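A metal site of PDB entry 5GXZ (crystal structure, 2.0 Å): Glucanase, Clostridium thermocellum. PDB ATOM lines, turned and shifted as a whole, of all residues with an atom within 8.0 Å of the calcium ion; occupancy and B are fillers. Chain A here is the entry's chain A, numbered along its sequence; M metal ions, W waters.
The calcium ion is bound by the backbone carbonyl oxygen (O) of Asp 488 (2.3 Å), the backbone carbonyl oxygen (O) of Asp 566 (2.3 Å), the side-chain carboxylate (OE2) of Glu 491 (2.3 Å), water W1 (2.3 Å), the side-chain carboxylate (OD1) of Asp 570 (2.3 Å), the side-chain amide oxygen (OD1) of Asn 569 (2.3 Å) and the side-chain carboxylate (OE1) of Glu 491 (2.9 Å).
Of the 18 residues printed, 5 come within 4 Å of the calcium ion.
The side-chain hydroxyl (OG1) of Thr 490 lies within hydrogen-bond range of the side-chain carboxylate (OD1) of Asp 488 (2.7 Å).
OD1 of Asp 566 is in hydrogen-bond range of OG1 of Thr 568 (2.6 Å).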
ATOM      1  N   THR A 461     -13.626  12.128 -21.018  1.00  0.00           N
ATOM      2  CA  THR A 461     -14.778  12.839 -21.540  1.00  0.00           C
ATOM      3  C   THR A 461     -15.906  11.839 -21.823  1.00  0.00           C
ATOM      4  O   THR A 461     -15.665  10.804 -22.447  1.00  0.00           O
ATOM      5  CB  THR A 461     -14.448  13.585 -22.837  1.00  0.00           C
ATOM      6  OG1 THR A 461     -13.452  14.576 -22.579  1.00  0.00           O
ATOM      7  CG2 THR A 461     -15.709  14.253 -23.388  1.00  0.00           C
ATOM      8  N   TYR A 486     -13.898  13.749 -33.051  1.00  0.00           N
ATOM      9  CA  TYR A 486     -12.483  13.995 -33.307  1.00  0.00           C
ATOM     10  C   TYR A 486     -11.794  14.471 -32.059  1.00  0.00           C
ATOM     11  O   TYR A 486     -12.298  15.335 -31.355  1.00  0.00           O
ATOM     12  CB  TYR A 486     -12.262  15.026 -34.418  1.00  0.00           C
ATOM     13  CG  TYR A 486     -12.805  14.595 -35.765  1.00  0.00           C
ATOM     14  CD1 TYR A 486     -12.059  13.732 -36.572  1.00  0.00           C
ATOM     15  CD2 TYR A 486     -14.061  14.997 -36.203  1.00  0.00           C
ATOM     16  CE1 TYR A 486     -12.542  13.316 -37.811  1.00  0.00           C
ATOM     17  CE2 TYR A 486     -14.553  14.571 -37.435  1.00  0.00           C
ATOM     18  CZ  TYR A 486     -13.772  13.746 -38.237  1.00  0.00           C
ATOM     19  OH  TYR A 486     -14.231  13.295 -39.449  1.00  0.00           O
ATOM     20  N   MET A 487     -10.600  13.924 -31.824  1.00  0.00           N
ATOM     21  CA  MET A 487      -9.780  14.312 -30.699  1.00  0.00           C
ATOM     22  C   MET A 487      -8.369  14.638 -31.176  1.00  0.00           C
ATOM     23  O   MET A 487      -7.882  14.095 -32.170  1.00  0.00           O
ATOM     24  CB  MET A 487      -9.647  13.168 -29.709  1.00  0.00           C
ATOM     25  CG  MET A 487     -10.956  12.527 -29.290  1.00  0.00           C
ATOM     26  SD  MET A 487     -10.578  10.858 -28.707  1.00  0.00           S
ATOM     27  CE  MET A 487     -10.907   9.851 -30.155  1.00  0.00           C
ATOM     28  N   ASP A 488      -7.725  15.488 -30.389  1.00  0.00           N
ATOM     29  CA  ASP A 488      -6.286  15.707 -30.458  1.00  0.00           C
ATOM     30  C   ASP A 488      -5.651  14.935 -29.290  1.00  0.00           C
ATOM     31  O   ASP A 488      -5.948  15.219 -28.137  1.00  0.00           O
ATOM     32  CB  ASP A 488      -6.024  17.209 -30.353  1.00  0.00           C
ATOM     33  CG  ASP A 488      -4.572  17.566 -30.544  1.00  0.00           C
ATOM     34  OD1 ASP A 488      -3.707  16.669 -30.451  1.00  0.00           O
ATOM     35  OD2 ASP A 488      -4.279  18.763 -30.748  1.00  0.00           O
ATOM     36  N   LEU A 489      -4.790  13.964 -29.571  1.00  0.00           N
ATOM     37  CA  LEU A 489      -4.142  13.197 -28.514  1.00  0.00           C
ATOM     38  C   LEU A 489      -2.719  13.657 -28.153  1.00  0.00           C
ATOM     39  O   LEU A 489      -1.972  12.929 -27.497  1.00  0.00           O
ATOM     40  CB  LEU A 489      -4.127  11.714 -28.889  1.00  0.00           C
ATOM     41  CG  LEU A 489      -5.456  10.998 -29.191  1.00  0.00           C
ATOM     42  CD1 LEU A 489      -5.155   9.540 -29.478  1.00  0.00           C
ATOM     43  CD2 LEU A 489      -6.432  11.168 -28.049  1.00  0.00           C
ATOM     44  N   THR A 490      -2.354  14.868 -28.559  1.00  0.00           N
ATOM     45  CA  THR A 490      -1.029  15.401 -28.219  1.00  0.00           C
ATOM     46  C   THR A 490      -0.636  15.236 -26.749  1.00  0.00           C
ATOM     47  O   THR A 490       0.459  14.769 -26.450  1.00  0.00           O
ATOM     48  CB  THR A 490      -0.863  16.882 -28.616  1.00  0.00           C
ATOM     49  OG1 THR A 490      -1.041  17.011 -30.035  1.00  0.00           O
ATOM     50  CG2 THR A 490       0.532  17.372 -28.263  1.00  0.00           C
ATOM     51  N   GLU A 491      -1.545  15.608 -25.839  1.00  0.00           N
ATOM     52  CA  GLU A 491      -1.233  15.564 -24.407  1.00  0.00           C
ATOM     53  C   GLU A 491      -1.011  14.143 -23.896  1.00  0.00           C
ATOM     54  O   GLU A 491      -0.317  13.944 -22.903  1.00  0.00           O
ATOM     55  CB  GLU A 491      -2.290  16.310 -23.579  1.00  0.00           C
ATOM     56  CG  GLU A 491      -3.669  15.637 -23.451  1.00  0.00           C
ATOM     57  CD  GLU A 491      -4.551  15.805 -24.672  1.00  0.00           C
ATOM     58  OE1 GLU A 491      -4.210  16.575 -25.596  1.00  0.00           O
ATOM     59  OE2 GLU A 491      -5.612  15.146 -24.715  1.00  0.00           O
ATOM     60  N   VAL A 492      -1.599  13.172 -24.587  1.00  0.00           N
ATOM     61  CA  VAL A 492      -1.505  11.768 -24.241  1.00  0.00           C
ATOM     62  C   VAL A 492      -0.075  11.307 -24.486  1.00  0.00           C
ATOM     63  O   VAL A 492       0.587  10.799 -23.573  1.00  0.00           O
ATOM     64  CB  VAL A 492      -2.511  10.927 -25.058  1.00  0.00           C
ATOM     65  CG1 VAL A 492      -2.428   9.467 -24.727  1.00  0.00           C
ATOM     66  CG2 VAL A 492      -3.927  11.431 -24.811  1.00  0.00           C
ATOM     67  N   ASN A 526      -1.552  14.247 -34.745  1.00  0.00           N
ATOM     68  CA  ASN A 526      -2.058  13.696 -33.485  1.00  0.00           C
ATOM     69  C   ASN A 526      -3.584  13.764 -33.392  1.00  0.00           C
ATOM     70  O   ASN A 526      -4.153  13.655 -32.298  1.00  0.00           O
ATOM     71  CB  ASN A 526      -1.424  14.394 -32.266  1.00  0.00           C
ATOM     72  CG  ASN A 526       0.086  14.273 -32.228  1.00  0.00           C
ATOM     73  OD1 ASN A 526       0.665  13.300 -32.694  1.00  0.00           O
ATOM     74  ND2 ASN A 526       0.737  15.271 -31.644  1.00  0.00           N
ATOM     75  N   PHE A 564      -3.411  13.901 -17.343  1.00  0.00           N
ATOM     76  CA  PHE A 564      -3.140  14.582 -18.624  1.00  0.00           C
ATOM     77  C   PHE A 564      -4.341  14.890 -19.523  1.00  0.00           C
ATOM     78  O   PHE A 564      -4.267  15.821 -20.330  1.00  0.00           O
ATOM     79  CB  PHE A 564      -2.084  13.836 -19.452  1.00  0.00           C
ATOM     80  CG  PHE A 564      -2.448  12.410 -19.755  1.00  0.00           C
ATOM     81  CD1 PHE A 564      -3.329  12.098 -20.788  1.00  0.00           C
ATOM     82  CD2 PHE A 564      -1.899  11.375 -19.010  1.00  0.00           C
ATOM     83  CE1 PHE A 564      -3.671  10.783 -21.061  1.00  0.00           C
ATOM     84  CE2 PHE A 564      -2.234  10.053 -19.282  1.00  0.00           C
ATOM     85  CZ  PHE A 564      -3.126   9.743 -20.296  1.00  0.00           C
ATOM     86  N   TRP A 565      -5.411  14.112 -19.429  1.00  0.00           N
ATOM     87  CA  TRP A 565      -6.481  14.169 -20.438  1.00  0.00           C
ATOM     88  C   TRP A 565      -6.934  15.606 -20.663  1.00  0.00           C
ATOM     89  O   TRP A 565      -7.278  16.323 -19.727  1.00  0.00           O
ATOM     90  CB  TRP A 565      -7.649  13.268 -20.026  1.00  0.00           C
ATOM     91  CG  TRP A 565      -8.763  13.217 -21.017  1.00  0.00           C
ATOM     92  CD1 TRP A 565      -9.993  13.797 -20.895  1.00  0.00           C
ATOM     93  CD2 TRP A 565      -8.765  12.541 -22.275  1.00  0.00           C
ATOM     94  NE1 TRP A 565     -10.754  13.531 -22.001  1.00  0.00           N
ATOM     95  CE2 TRP A 565     -10.029  12.766 -22.861  1.00  0.00           C
ATOM     96  CE3 TRP A 565      -7.820  11.771 -22.962  1.00  0.00           C
ATOM     97  CZ2 TRP A 565     -10.365  12.244 -24.110  1.00  0.00           C
ATOM     98  CZ3 TRP A 565      -8.158  11.246 -24.202  1.00  0.00           C
ATOM     99  CH2 TRP A 565      -9.419  11.487 -24.762  1.00  0.00           C
ATOM    100  N   ASP A 566      -6.895  16.050 -21.916  1.00  0.00           N
ATOM    101  CA  ASP A 566      -7.285  17.428 -22.217  1.00  0.00           C
ATOM    102  C   ASP A 566      -8.276  17.474 -23.382  1.00  0.00           C
ATOM    103  O   ASP A 566      -7.886  17.366 -24.550  1.00  0.00           O
ATOM    104  CB  ASP A 566      -6.066  18.332 -22.474  1.00  0.00           C
ATOM    105  CG  ASP A 566      -6.447  19.762 -22.781  1.00  0.00           C
ATOM    106  OD1 ASP A 566      -7.612  20.174 -22.606  1.00  0.00           O
ATOM    107  OD2 ASP A 566      -5.557  20.513 -23.237  1.00  0.00           O
ATOM    108  N   PRO A 567      -9.559  17.648 -23.055  1.00  0.00           N
ATOM    109  CA  PRO A 567     -10.566  17.789 -24.096  1.00  0.00           C
ATOM    110  C   PRO A 567     -10.589  19.169 -24.759  1.00  0.00           C
ATOM    111  O   PRO A 567     -11.140  19.291 -25.860  1.00  0.00           O
ATOM    112  CB  PRO A 567     -11.876  17.543 -23.342  1.00  0.00           C
ATOM    113  CG  PRO A 567     -11.587  18.051 -21.948  1.00  0.00           C
ATOM    114  CD  PRO A 567     -10.120  17.798 -21.698  1.00  0.00           C
ATOM    115  N   THR A 568     -10.019  20.196 -24.130  1.00  0.00           N
ATOM    116  CA  THR A 568     -10.094  21.571 -24.658  1.00  0.00           C
ATOM    117  C   THR A 568      -9.394  21.762 -26.012  1.00  0.00           C
ATOM    118  O   THR A 568      -9.604  22.777 -26.681  1.00  0.00           O
ATOM    119  CB  THR A 568      -9.588  22.660 -23.681  1.00  0.00           C
ATOM    120  OG1 THR A 568      -8.168  22.521 -23.495  1.00  0.00           O
ATOM    121  CG2 THR A 568     -10.317  22.599 -22.331  1.00  0.00           C
ATOM    122  N   ASN A 569      -8.555  20.803 -26.408  1.00  0.00           N
ATOM    123  CA  ASN A 569      -7.957  20.809 -27.741  1.00  0.00           C
ATOM    124  C   ASN A 569      -8.581  19.799 -28.710  1.00  0.00           C
ATOM    125  O   ASN A 569      -8.057  19.596 -29.814  1.00  0.00           O
ATOM    126  CB  ASN A 569      -6.436  20.653 -27.678  1.00  0.00           C
ATOM    127  CG  ASN A 569      -5.983  19.316 -27.096  1.00  0.00           C
ATOM    128  OD1 ASN A 569      -6.769  18.383 -26.926  1.00  0.00           O
ATOM    129  ND2 ASN A 569      -4.690  19.212 -26.809  1.00  0.00           N
ATOM    130  N   ASP A 570      -9.683  19.163 -28.326  1.00  0.00           N
ATOM    131  CA  ASP A 570     -10.331  18.196 -29.205  1.00  0.00           C
ATOM    132  C   ASP A 570     -11.327  18.904 -30.118  1.00  0.00           C
ATOM    133  O   ASP A 570     -12.253  19.543 -29.647  1.00  0.00           O
ATOM    134  CB  ASP A 570     -11.029  17.091 -28.393  1.00  0.00           C
ATOM    135  CG  ASP A 570     -10.051  16.208 -27.609  1.00  0.00           C
ATOM    136  OD1 ASP A 570      -8.802  16.342 -27.733  1.00  0.00           O
ATOM    137  OD2 ASP A 570     -10.573  15.369 -26.838  1.00  0.00           O
ATOM    138  N   PHE A 571     -11.140  18.744 -31.427  1.00  0.00           N
ATOM    139  CA  PHE A 571     -12.021  19.316 -32.447  1.00  0.00           C
ATOM    140  C   PHE A 571     -13.518  19.154 -32.102  1.00  0.00           C
ATOM    141  O   PHE A 571     -14.267  20.128 -32.125  1.00  0.00           O
ATOM    142  CB  PHE A 571     -11.691  18.665 -33.797  1.00  0.00           C
ATOM    143  CG  PHE A 571     -12.481  19.180 -34.960  1.00  0.00           C
ATOM    144  CD1 PHE A 571     -12.036  20.273 -35.684  1.00  0.00           C
ATOM    145  CD2 PHE A 571     -13.658  18.560 -35.358  1.00  0.00           C
ATOM    146  CE1 PHE A 571     -12.760  20.752 -36.770  1.00  0.00           C
ATOM    147  CE2 PHE A 571     -14.389  19.033 -36.448  1.00  0.00           C
ATOM    148  CZ  PHE A 571     -13.932  20.123 -37.159  1.00  0.00           C
ATOM    149  N   TYR A 573     -15.030  18.614 -29.274  1.00  0.00           N
ATOM    150  CA  TYR A 573     -15.435  19.188 -27.986  1.00  0.00           C
ATOM    151  C   TYR A 573     -15.776  20.666 -28.077  1.00  0.00           C
ATOM    152  O   TYR A 573     -16.478  21.189 -27.209  1.00  0.00           O
ATOM    153  CB  TYR A 573     -14.320  18.987 -26.972  1.00  0.00           C
ATOM    154  CG  TYR A 573     -14.671  18.991 -25.499  1.00  0.00           C
ATOM    155  CD1 TYR A 573     -15.364  17.931 -24.916  1.00  0.00           C
ATOM    156  CD2 TYR A 573     -14.210  20.008 -24.662  1.00  0.00           C
ATOM    157  CE1 TYR A 573     -15.636  17.909 -23.561  1.00  0.00           C
ATOM    158  CE2 TYR A 573     -14.484  19.997 -23.294  1.00  0.00           C
ATOM    159  CZ  TYR A 573     -15.177  18.939 -22.752  1.00  0.00           C
ATOM    160  OH  TYR A 573     -15.435  18.931 -21.391  1.00  0.00           O
HETATM  161 CA    CA M   1      -6.980  16.148 -26.300  1.00  0.00          CA
HETATM  162  O   HOH W   1      -8.296  14.314 -25.752  1.00  0.00           O
